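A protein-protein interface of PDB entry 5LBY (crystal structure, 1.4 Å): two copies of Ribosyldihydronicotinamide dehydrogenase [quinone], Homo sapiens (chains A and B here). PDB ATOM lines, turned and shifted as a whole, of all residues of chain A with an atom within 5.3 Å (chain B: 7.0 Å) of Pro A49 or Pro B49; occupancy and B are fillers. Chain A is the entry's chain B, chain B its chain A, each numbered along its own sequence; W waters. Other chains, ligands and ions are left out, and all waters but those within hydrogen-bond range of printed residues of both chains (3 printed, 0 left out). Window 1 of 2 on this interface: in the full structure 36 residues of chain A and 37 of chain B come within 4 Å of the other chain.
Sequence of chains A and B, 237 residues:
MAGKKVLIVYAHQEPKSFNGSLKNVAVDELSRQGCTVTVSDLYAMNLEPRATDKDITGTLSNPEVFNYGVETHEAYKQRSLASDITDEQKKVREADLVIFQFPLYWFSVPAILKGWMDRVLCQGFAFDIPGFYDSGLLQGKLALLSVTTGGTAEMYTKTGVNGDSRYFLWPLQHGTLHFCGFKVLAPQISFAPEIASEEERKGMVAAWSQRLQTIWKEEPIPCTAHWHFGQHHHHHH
NH2 of Arg A50 sits at hydrogen-bond distance from O of Asn B46 (3.0 Å). NE of Arg A50 lies within hydrogen-bond range of O of Leu B47, at 2.9 Å. The backbone carbonyl oxygen (O) of Leu A47 lies within hydrogen-bond range of the guanidinium group (NE) of Arg B50 (2.9 Å). The side-chain carboxylate (OD2) of Asp A118 is in hydrogen-bond range of the backbone NH (N) of Ala B111 (2.9 Å). The side-chain carboxylate (OD2) of Asp B118 is in hydrogen-bond range of the backbone NH (N) of Ala A111 (2.9 Å).
The side-chain carboxylate (OE2) of Glu B48 lies within salt-bridge range of the guanidinium group (NH1) of Arg B50, 2.9 Å away. O of Glu B48 is in hydrogen-bond range of NH1 of Arg B119 (2.9 Å). The side-chain amino group (NZ) of Lys B114 lies within salt-bridge range of the side-chain carboxylate (OD1) of Asp B118 (2.7 Å). NH1 of Arg A50 is in salt-bridge range of OE2 of Glu A48 (2.9 Å). The guanidinium group of Arg A119 sits at hydrogen-bond distance from the backbone carbonyl oxygen of Glu A48 (2.9 Å).
Among the printed residues, pairs that only touch across the chains: Ala A51 with Tyr B43 (3.3 Å), Pro A49 with Ala B111 (3.4 Å), Ala A111 with Pro B49 (3.4 Å), Gly A115 with Ala B111 (3.4 Å), Ala A111 with Gly B115 (3.4 Å), Glu A48 with Arg B50 (3.5 Å), Arg A50 with Glu B48 (3.5 Å), Ala A111 with Ala B111 (3.7 Å), Arg A50 with Pro B49 (3.7 Å), Pro A49 with Arg B50 (3.7 Å), Asp A118 with Pro B110 (3.8 Å), Ala A111 with Lys B114 (3.9 Å) and Pro A49 with Pro B49 (3.98 Å).
Pro A49 touches just these residues of chain B: Pro B49 (3.98 Å), Arg B50 (3.7 Å) and Ala B111 (3.4 Å). Pro B49 touches just these residues of chain A: Pro A49, Arg A50 and Ala A111. Printed residues of chain A within 4 Å of Gly B115: Ala A111. Printed residues of chain A within 4 Å of Tyr B43: Ala A51. Of the printed residues of chain B, Arg A50 touches Asn B46, Leu B47, Glu B48 and Pro B49. The nearest residue of chain B that does not touch Pro A49 is Ile B112 (4.9 Å).
Of the 19 printed residues of chain B, 11 touch a printed residue of chain A. Printed residues of chain B that touch a printed residue of chain A: Tyr B43, Asn B46, Leu B47, Glu B48, Pro B49, Arg B50, Pro B110, Ala B111, Lys B114, Gly B115 and Asp B118. Printed residues of chain A that touch a printed residue of chain B: Leu A47, Glu A48, Pro A49, Arg A50, Ala A51, Ala A111, Gly A115 and Asp A118. Hydrophobic or aromatic side chains of chain A that line the printed part of chain B: Pro A49 and Ala A111. Among the printed residues, 18 pairs touch across the chains. Among the printed residues, no Asp or Glu carboxylate lies within 4 Å of a Lys or Arg side-chain nitrogen of the other chain.
Pro A49 touches Arg B50, and with the chains exchanged Arg A50 touches Pro B49. Pro A49 touches Ala B111, and with the chains exchanged Ala A111 touches Pro B49. Ala A111 touches its own counterpart, Ala B111. Ala A111 touches Asp B118, and with the chains exchanged Asp A118 touches Ala B111. Positions printed for both chains: 47, 48, 49, 50, 51, 111, 112, 115, 116, 118 and 119. Of the 18 pairs that touch across the chains among the printed residues, 14 have their exchanged pair printed and touching as well.
Water W1 lies within hydrogen-bond range of OH of Tyr B43, N of Ile B112 and N of Ala A51. Water W3 lies within hydrogen-bond range of the guanidinium group (NH2) of Arg B50 (2.9 Å), the side-chain carboxylate (OE1) of Glu A48 (2.9 Å) and the guanidinium group (NH1) of Arg A50 (3.4 Å). Water W2 bridges N of Ile A112 (3.0 Å) and N of Ala B51 (3.4 Å).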
ATOM      1  N   LEU A  47      19.481 -19.476   5.169  1.00  0.00           N
ATOM      2  CA  LEU A  47      19.287 -18.150   5.745  1.00  0.00           C
ATOM      3  C   LEU A  47      19.811 -18.095   7.182  1.00  0.00           C
ATOM      4  O   LEU A  47      19.462 -18.904   8.012  1.00  0.00           O
ATOM      5  CB  LEU A  47      17.814 -17.755   5.749  1.00  0.00           C
ATOM      6  CG  LEU A  47      17.538 -16.317   6.151  1.00  0.00           C
ATOM      7  CD1 LEU A  47      17.709 -15.370   4.978  1.00  0.00           C
ATOM      8  CD2 LEU A  47      16.130 -16.169   6.724  1.00  0.00           C
ATOM      9  N   GLU A  48      20.588 -17.057   7.439  1.00  0.00           N
ATOM     10  CA  GLU A  48      21.086 -16.745   8.793  1.00  0.00           C
ATOM     11  C   GLU A  48      19.874 -16.352   9.671  1.00  0.00           C
ATOM     12  O   GLU A  48      19.161 -15.411   9.360  1.00  0.00           O
ATOM     13  CB  GLU A  48      22.056 -15.552   8.733  1.00  0.00           C
ATOM     14  CG  GLU A  48      22.443 -15.035  10.096  1.00  0.00           C
ATOM     15  CD  GLU A  48      23.229 -16.065  10.879  1.00  0.00           C
ATOM     16  OE1 GLU A  48      24.387 -16.345  10.491  1.00  0.00           O
ATOM     17  OE2 GLU A  48      22.699 -16.602  11.868  1.00  0.00           O
ATOM     18  N   PRO A  49      19.622 -17.049  10.776  1.00  0.00           N
ATOM     19  CA  PRO A  49      18.532 -16.636  11.651  1.00  0.00           C
ATOM     20  C   PRO A  49      18.936 -15.707  12.778  1.00  0.00           C
ATOM     21  O   PRO A  49      18.069 -15.075  13.345  1.00  0.00           O
ATOM     22  CB  PRO A  49      18.039 -17.960  12.249  1.00  0.00           C
ATOM     23  CG  PRO A  49      18.627 -19.024  11.391  1.00  0.00           C
ATOM     24  CD  PRO A  49      19.955 -18.469  10.968  1.00  0.00           C
ATOM     25  N   ARG A  50      20.215 -15.664  13.124  1.00  0.00           N
ATOM     26  CA  ARG A  50      20.682 -14.934  14.292  1.00  0.00           C
ATOM     27  C   ARG A  50      20.711 -13.445  14.003  1.00  0.00           C
ATOM     28  O   ARG A  50      21.199 -13.050  12.960  1.00  0.00           O
ATOM     29  CB  ARG A  50      22.061 -15.405  14.740  1.00  0.00           C
ATOM     30  CG  ARG A  50      22.177 -16.913  14.989  1.00  0.00           C
ATOM     31  CD  ARG A  50      23.641 -17.227  15.229  1.00  0.00           C
ATOM     32  NE  ARG A  50      23.989 -18.647  15.200  1.00  0.00           N
ATOM     33  CZ  ARG A  50      24.446 -19.283  14.146  1.00  0.00           C
ATOM     34  NH1 ARG A  50      24.382 -18.753  12.931  1.00  0.00           N
ATOM     35  NH2 ARG A  50      24.901 -20.495  14.282  1.00  0.00           N
ATOM     36  N   ALA A  51      20.311 -12.652  14.986  1.00  0.00           N
ATOM     37  CA  ALA A  51      20.404 -11.186  14.887  1.00  0.00           C
ATOM     38  C   ALA A  51      21.780 -10.786  15.421  1.00  0.00           C
ATOM     39  O   ALA A  51      22.002 -10.778  16.636  1.00  0.00           O
ATOM     40  CB  ALA A  51      19.302 -10.506  15.722  1.00  0.00           C
ATOM     41  N   ALA A 111      12.514 -21.744  13.687  1.00  0.00           N
ATOM     42  CA  ALA A 111      13.466 -20.676  13.972  1.00  0.00           C
ATOM     43  C   ALA A 111      14.036 -19.983  12.728  1.00  0.00           C
ATOM     44  O   ALA A 111      14.329 -18.794  12.785  1.00  0.00           O
ATOM     45  CB  ALA A 111      14.614 -21.191  14.835  1.00  0.00           C
ATOM     46  N   ILE A 112      14.259 -20.738  11.627  1.00  0.00           N
ATOM     47  CA  ILE A 112      14.816 -20.047  10.476  1.00  0.00           C
ATOM     48  C   ILE A 112      13.862 -18.936   9.938  1.00  0.00           C
ATOM     49  O   ILE A 112      14.339 -17.899   9.469  1.00  0.00           O
ATOM     50  CB  ILE A 112      15.192 -21.070   9.356  1.00  0.00           C
ATOM     51  CG1 ILE A 112      16.120 -20.450   8.321  1.00  0.00           C
ATOM     52  CG2 ILE A 112      13.949 -21.658   8.698  1.00  0.00           C
ATOM     53  CD1 ILE A 112      16.700 -21.466   7.372  1.00  0.00           C
ATOM     54  N   GLY A 115      13.876 -16.019  12.248  1.00  0.00           N
ATOM     55  CA  GLY A 115      15.017 -15.185  11.926  1.00  0.00           C
ATOM     56  C   GLY A 115      14.779 -14.269  10.748  1.00  0.00           C
ATOM     57  O   GLY A 115      15.207 -13.119  10.745  1.00  0.00           O
ATOM     58  N   TRP A 116      14.071 -14.793   9.721  1.00  0.00           N
ATOM     59  CA  TRP A 116      13.644 -13.934   8.606  1.00  0.00           C
ATOM     60  C   TRP A 116      12.821 -12.773   9.170  1.00  0.00           C
ATOM     61  O   TRP A 116      13.047 -11.608   8.802  1.00  0.00           O
ATOM     62  CB  TRP A 116      12.835 -14.753   7.613  1.00  0.00           C
ATOM     63  CG  TRP A 116      12.463 -14.074   6.326  1.00  0.00           C
ATOM     64  CD1 TRP A 116      13.122 -14.183   5.115  1.00  0.00           C
ATOM     65  CD2 TRP A 116      11.346 -13.225   6.103  1.00  0.00           C
ATOM     66  NE1 TRP A 116      12.466 -13.456   4.153  1.00  0.00           N
ATOM     67  CE2 TRP A 116      11.384 -12.847   4.728  1.00  0.00           C
ATOM     68  CE3 TRP A 116      10.304 -12.736   6.907  1.00  0.00           C
ATOM     69  CZ2 TRP A 116      10.438 -11.998   4.179  1.00  0.00           C
ATOM     70  CZ3 TRP A 116       9.385 -11.893   6.352  1.00  0.00           C
ATOM     71  CH2 TRP A 116       9.459 -11.527   4.996  1.00  0.00           C
ATOM     72  N   ASP A 118      12.727 -11.473  12.250  1.00  0.00           N
ATOM     73  CA  ASP A 118      13.547 -10.622  13.107  1.00  0.00           C
ATOM     74  C   ASP A 118      14.479  -9.691  12.323  1.00  0.00           C
ATOM     75  O   ASP A 118      14.686  -8.555  12.736  1.00  0.00           O
ATOM     76  CB  ASP A 118      14.441 -11.498  13.999  1.00  0.00           C
ATOM     77  CG  ASP A 118      13.728 -12.310  15.071  1.00  0.00           C
ATOM     78  OD1 ASP A 118      12.516 -12.052  15.315  1.00  0.00           O
ATOM     79  OD2 ASP A 118      14.355 -13.183  15.680  1.00  0.00           O
ATOM     80  N   ARG A 119      15.041 -10.227  11.237  1.00  0.00           N
ATOM     81  CA  ARG A 119      16.090  -9.516  10.526  1.00  0.00           C
ATOM     82  C   ARG A 119      15.566  -8.693   9.347  1.00  0.00           C
ATOM     83  O   ARG A 119      16.116  -7.638   9.039  1.00  0.00           O
ATOM     84  CB  ARG A 119      17.099 -10.563  10.011  1.00  0.00           C
ATOM     85  CG  ARG A 119      17.865 -11.282  11.127  1.00  0.00           C
ATOM     86  CD  ARG A 119      18.734 -12.386  10.607  1.00  0.00           C
ATOM     87  NE  ARG A 119      19.910 -11.913   9.898  1.00  0.00           N
ATOM     88  CZ  ARG A 119      20.206 -12.124   8.633  1.00  0.00           C
ATOM     89  NH1 ARG A 119      19.431 -12.917   7.904  1.00  0.00           N
ATOM     90  NH2 ARG A 119      21.266 -11.552   8.105  1.00  0.00           N
ATOM     91  N   TYR B  43      24.269 -16.470  22.021  1.00  0.00           N
ATOM     92  CA  TYR B  43      25.031 -15.755  21.012  1.00  0.00           C
ATOM     93  C   TYR B  43      26.530 -16.007  21.141  1.00  0.00           C
ATOM     94  O   TYR B  43      27.224 -16.158  20.141  1.00  0.00           O
ATOM     95  CB  TYR B  43      24.763 -14.257  21.048  1.00  0.00           C
ATOM     96  CG  TYR B  43      23.399 -13.874  20.552  1.00  0.00           C
ATOM     97  CD1 TYR B  43      23.141 -13.760  19.192  1.00  0.00           C
ATOM     98  CD2 TYR B  43      22.374 -13.559  21.411  1.00  0.00           C
ATOM     99  CE1 TYR B  43      21.905 -13.376  18.724  1.00  0.00           C
ATOM    100  CE2 TYR B  43      21.145 -13.126  20.953  1.00  0.00           C
ATOM    101  CZ  TYR B  43      20.916 -13.046  19.603  1.00  0.00           C
ATOM    102  OH  TYR B  43      19.660 -12.610  19.185  1.00  0.00           O
ATOM    103  N   ASN B  46      27.398 -19.119  19.631  1.00  0.00           N
ATOM    104  CA  ASN B  46      27.022 -19.141  18.238  1.00  0.00           C
ATOM    105  C   ASN B  46      26.067 -20.304  17.953  1.00  0.00           C
ATOM    106  O   ASN B  46      26.153 -20.990  16.952  1.00  0.00           O
ATOM    107  CB  ASN B  46      28.225 -19.176  17.299  1.00  0.00           C
ATOM    108  CG  ASN B  46      27.876 -18.756  15.911  1.00  0.00           C
ATOM    109  OD1 ASN B  46      26.992 -17.873  15.713  1.00  0.00           O
ATOM    110  ND2 ASN B  46      28.498 -19.379  14.959  1.00  0.00           N
ATOM    111  N   LEU B  47      25.088 -20.503  18.829  1.00  0.00           N
ATOM    112  CA  LEU B  47      24.197 -21.623  18.711  1.00  0.00           C
ATOM    113  C   LEU B  47      23.535 -21.673  17.349  1.00  0.00           C
ATOM    114  O   LEU B  47      22.942 -20.688  16.902  1.00  0.00           O
ATOM    115  CB  LEU B  47      23.117 -21.585  19.805  1.00  0.00           C
ATOM    116  CG  LEU B  47      22.249 -22.835  19.875  1.00  0.00           C
ATOM    117  CD1 LEU B  47      22.897 -23.826  20.831  1.00  0.00           C
ATOM    118  CD2 LEU B  47      20.864 -22.506  20.392  1.00  0.00           C
ATOM    119  N   GLU B  48      23.573 -22.852  16.747  1.00  0.00           N
ATOM    120  CA  GLU B  48      22.883 -23.112  15.505  1.00  0.00           C
ATOM    121  C   GLU B  48      21.356 -23.052  15.723  1.00  0.00           C
ATOM    122  O   GLU B  48      20.848 -23.797  16.550  1.00  0.00           O
ATOM    123  CB  GLU B  48      23.295 -24.457  14.920  1.00  0.00           C
ATOM    124  CG  GLU B  48      22.438 -24.951  13.759  1.00  0.00           C
ATOM    125  CD  GLU B  48      22.623 -24.108  12.516  1.00  0.00           C
ATOM    126  OE1 GLU B  48      23.768 -24.140  11.990  1.00  0.00           O
ATOM    127  OE2 GLU B  48      21.714 -23.369  12.146  1.00  0.00           O
ATOM    128  N   PRO B  49      20.608 -22.199  15.012  1.00  0.00           N
ATOM    129  CA  PRO B  49      19.160 -22.182  15.215  1.00  0.00           C
ATOM    130  C   PRO B  49      18.378 -23.057  14.280  1.00  0.00           C
ATOM    131  O   PRO B  49      17.207 -23.369  14.542  1.00  0.00           O
ATOM    132  CB  PRO B  49      18.766 -20.715  15.021  1.00  0.00           C
ATOM    133  CG  PRO B  49      20.053 -19.968  15.064  1.00  0.00           C
ATOM    134  CD  PRO B  49      21.092 -20.907  14.495  1.00  0.00           C
ATOM    135  N   ARG B  50      18.969 -23.395  13.136  1.00  0.00           N
ATOM    136  CA  ARG B  50      18.235 -24.077  12.077  1.00  0.00           C
ATOM    137  C   ARG B  50      18.081 -25.546  12.406  1.00  0.00           C
ATOM    138  O   ARG B  50      19.013 -26.207  12.843  1.00  0.00           O
ATOM    139  CB  ARG B  50      18.966 -23.946  10.749  1.00  0.00           C
ATOM    140  CG  ARG B  50      19.309 -22.556  10.311  1.00  0.00           C
ATOM    141  CD  ARG B  50      20.152 -22.594   9.086  1.00  0.00           C
ATOM    142  NE  ARG B  50      20.800 -21.357   8.699  1.00  0.00           N
ATOM    143  CZ  ARG B  50      22.015 -20.955   9.094  1.00  0.00           C
ATOM    144  NH1 ARG B  50      22.666 -21.569  10.022  1.00  0.00           N
ATOM    145  NH2 ARG B  50      22.531 -19.927   8.514  1.00  0.00           N
ATOM    146  N   ALA B  51      16.910 -26.093  12.077  1.00  0.00           N
ATOM    147  CA  ALA B  51      16.633 -27.546  12.225  1.00  0.00           C
ATOM    148  C   ALA B  51      17.068 -28.209  10.943  1.00  0.00           C
ATOM    149  O   ALA B  51      16.364 -28.176   9.945  1.00  0.00           O
ATOM    150  CB  ALA B  51      15.168 -27.757  12.496  1.00  0.00           C
ATOM    151  N   THR B  52      18.241 -28.861  10.967  1.00  0.00           N
ATOM    152  CA  THR B  52      18.769 -29.463   9.738  1.00  0.00           C
ATOM    153  C   THR B  52      19.343 -30.843  10.021  1.00  0.00           C
ATOM    154  O   THR B  52      19.479 -31.265  11.191  1.00  0.00           O
ATOM    155  CB  THR B  52      19.877 -28.617   9.088  1.00  0.00           C
ATOM    156  OG1 THR B  52      21.138 -28.814   9.781  1.00  0.00           O
ATOM    157  CG2 THR B  52      19.477 -27.161   9.013  1.00  0.00           C
ATOM    158  N   ASP B  55      21.958 -31.984  12.661  1.00  0.00           N
ATOM    159  CA  ASP B  55      21.615 -32.299  14.017  1.00  0.00           C
ATOM    160  C   ASP B  55      21.739 -33.774  14.370  1.00  0.00           C
ATOM    161  O   ASP B  55      21.650 -34.151  15.544  1.00  0.00           O
ATOM    162  CB  ASP B  55      20.215 -31.758  14.349  1.00  0.00           C
ATOM    163  CG  ASP B  55      20.184 -30.252  14.338  1.00  0.00           C
ATOM    164  OD1 ASP B  55      21.281 -29.621  14.230  1.00  0.00           O
ATOM    165  OD2 ASP B  55      19.083 -29.651  14.436  1.00  0.00           O
ATOM    166  N   ASP B  84      26.191 -30.312  20.418  1.00  0.00           N
ATOM    167  CA  ASP B  84      25.626 -29.062  20.976  1.00  0.00           C
ATOM    168  C   ASP B  84      24.261 -29.304  21.591  1.00  0.00           C
ATOM    169  O   ASP B  84      23.950 -28.817  22.685  1.00  0.00           O
ATOM    170  CB  ASP B  84      25.628 -27.956  19.957  1.00  0.00           C
ATOM    171  CG  ASP B  84      24.733 -28.222  18.749  1.00  0.00           C
ATOM    172  OD1 ASP B  84      24.553 -29.374  18.326  1.00  0.00           O
ATOM    173  OD2 ASP B  84      24.218 -27.203  18.187  1.00  0.00           O
ATOM    174  N   PRO B 110      13.766 -14.244  20.578  1.00  0.00           N
ATOM    175  CA  PRO B 110      14.686 -14.106  19.447  1.00  0.00           C
ATOM    176  C   PRO B 110      14.866 -15.427  18.742  1.00  0.00           C
ATOM    177  O   PRO B 110      14.877 -16.500  19.390  1.00  0.00           O
ATOM    178  CB  PRO B 110      15.987 -13.646  20.102  1.00  0.00           C
ATOM    179  CG  PRO B 110      15.550 -12.930  21.365  1.00  0.00           C
ATOM    180  CD  PRO B 110      14.368 -13.769  21.849  1.00  0.00           C
ATOM    181  N   ALA B 111      15.131 -15.395  17.449  1.00  0.00           N
ATOM    182  CA  ALA B 111      15.272 -16.642  16.685  1.00  0.00           C
ATOM    183  C   ALA B 111      16.322 -17.582  17.236  1.00  0.00           C
ATOM    184  O   ALA B 111      16.150 -18.790  17.139  1.00  0.00           O
ATOM    185  CB  ALA B 111      15.538 -16.335  15.214  1.00  0.00           C
ATOM    186  N   ILE B 112      17.432 -17.079  17.774  1.00  0.00           N
ATOM    187  CA  ILE B 112      18.458 -18.006  18.288  1.00  0.00           C
ATOM    188  C   ILE B 112      17.873 -18.832  19.421  1.00  0.00           C
ATOM    189  O   ILE B 112      18.225 -20.015  19.566  1.00  0.00           O
ATOM    190  CB  ILE B 112      19.755 -17.254  18.678  1.00  0.00           C
ATOM    191  CG1 ILE B 112      20.918 -18.214  18.770  1.00  0.00           C
ATOM    192  CG2 ILE B 112      19.590 -16.437  19.935  1.00  0.00           C
ATOM    193  CD1 ILE B 112      22.255 -17.537  18.978  1.00  0.00           C
ATOM    194  N   LEU B 113      17.044 -18.214  20.261  1.00  0.00           N
ATOM    195  CA  LEU B 113      16.380 -18.921  21.354  1.00  0.00           C
ATOM    196  C   LEU B 113      15.259 -19.834  20.829  1.00  0.00           C
ATOM    197  O   LEU B 113      15.071 -20.938  21.342  1.00  0.00           O
ATOM    198  CB  LEU B 113      15.907 -17.927  22.407  1.00  0.00           C
ATOM    199  CG  LEU B 113      15.132 -18.461  23.578  1.00  0.00           C
ATOM    200  CD1 LEU B 113      15.821 -19.630  24.268  1.00  0.00           C
ATOM    201  CD2 LEU B 113      14.852 -17.355  24.602  1.00  0.00           C
ATOM    202  N   LYS B 114      14.539 -19.405  19.815  1.00  0.00           N
ATOM    203  CA  LYS B 114      13.586 -20.282  19.199  1.00  0.00           C
ATOM    204  C   LYS B 114      14.294 -21.551  18.699  1.00  0.00           C
ATOM    205  O   LYS B 114      13.757 -22.656  18.784  1.00  0.00           O
ATOM    206  CB  LYS B 114      12.858 -19.608  18.038  1.00  0.00           C
ATOM    207  CG  LYS B 114      11.698 -20.460  17.447  1.00  0.00           C
ATOM    208  CD  LYS B 114      10.721 -20.934  18.499  1.00  0.00           C
ATOM    209  CE  LYS B 114       9.393 -21.392  17.947  1.00  0.00           C
ATOM    210  NZ  LYS B 114       9.545 -22.459  16.892  1.00  0.00           N
ATOM    211  N   GLY B 115      15.475 -21.394  18.136  1.00  0.00           N
ATOM    212  CA  GLY B 115      16.217 -22.546  17.638  1.00  0.00           C
ATOM    213  C   GLY B 115      16.668 -23.457  18.771  1.00  0.00           C
ATOM    214  O   GLY B 115      16.658 -24.692  18.585  1.00  0.00           O
ATOM    215  N   TRP B 116      17.051 -22.905  19.925  1.00  0.00           N
ATOM    216  CA  TRP B 116      17.300 -23.741  21.098  1.00  0.00           C
ATOM    217  C   TRP B 116      16.061 -24.585  21.406  1.00  0.00           C
ATOM    218  O   TRP B 116      16.171 -25.806  21.636  1.00  0.00           O
ATOM    219  CB  TRP B 116      17.687 -22.859  22.289  1.00  0.00           C
ATOM    220  CG  TRP B 116      18.137 -23.572  23.535  1.00  0.00           C
ATOM    221  CD1 TRP B 116      19.459 -23.776  23.905  1.00  0.00           C
ATOM    222  CD2 TRP B 116      17.328 -24.114  24.546  1.00  0.00           C
ATOM    223  NE1 TRP B 116      19.480 -24.409  25.131  1.00  0.00           N
ATOM    224  CE2 TRP B 116      18.197 -24.635  25.541  1.00  0.00           C
ATOM    225  CE3 TRP B 116      15.946 -24.151  24.773  1.00  0.00           C
ATOM    226  CZ2 TRP B 116      17.716 -25.239  26.706  1.00  0.00           C
ATOM    227  CZ3 TRP B 116      15.479 -24.802  25.922  1.00  0.00           C
ATOM    228  CH2 TRP B 116      16.357 -25.309  26.854  1.00  0.00           C
ATOM    229  N   ASP B 118      13.529 -25.445  19.427  1.00  0.00           N
ATOM    230  CA  ASP B 118      13.254 -26.375  18.327  1.00  0.00           C
ATOM    231  C   ASP B 118      14.170 -27.582  18.341  1.00  0.00           C
ATOM    232  O   ASP B 118      13.710 -28.697  18.030  1.00  0.00           O
ATOM    233  CB  ASP B 118      13.424 -25.656  16.994  1.00  0.00           C
ATOM    234  CG  ASP B 118      12.379 -24.554  16.683  1.00  0.00           C
ATOM    235  OD1 ASP B 118      11.361 -24.438  17.392  1.00  0.00           O
ATOM    236  OD2 ASP B 118      12.645 -23.848  15.666  1.00  0.00           O
ATOM    237  N   ARG B 119      15.429 -27.378  18.668  1.00  0.00           N
ATOM    238  CA  ARG B 119      16.443 -28.414  18.518  1.00  0.00           C
ATOM    239  C   ARG B 119      16.694 -29.202  19.799  1.00  0.00           C
ATOM    240  O   ARG B 119      16.985 -30.384  19.778  1.00  0.00           O
ATOM    241  CB  ARG B 119      17.746 -27.780  18.055  1.00  0.00           C
ATOM    242  CG  ARG B 119      17.679 -27.131  16.696  1.00  0.00           C
ATOM    243  CD  ARG B 119      18.925 -26.382  16.320  1.00  0.00           C
ATOM    244  NE  ARG B 119      20.065 -27.267  16.056  1.00  0.00           N
ATOM    245  CZ  ARG B 119      21.219 -27.306  16.726  1.00  0.00           C
ATOM    246  NH1 ARG B 119      21.438 -26.422  17.677  1.00  0.00           N
ATOM    247  NH2 ARG B 119      22.109 -28.210  16.440  1.00  0.00           N
HETATM  248  O   HOH W   1      18.517 -14.314  17.232  1.00  0.00           O
HETATM  249  O   HOH W   2      14.611 -23.701  11.562  1.00  0.00           O
HETATM  250  O   HOH W   3      24.987 -19.012   9.644  1.00  0.00           O
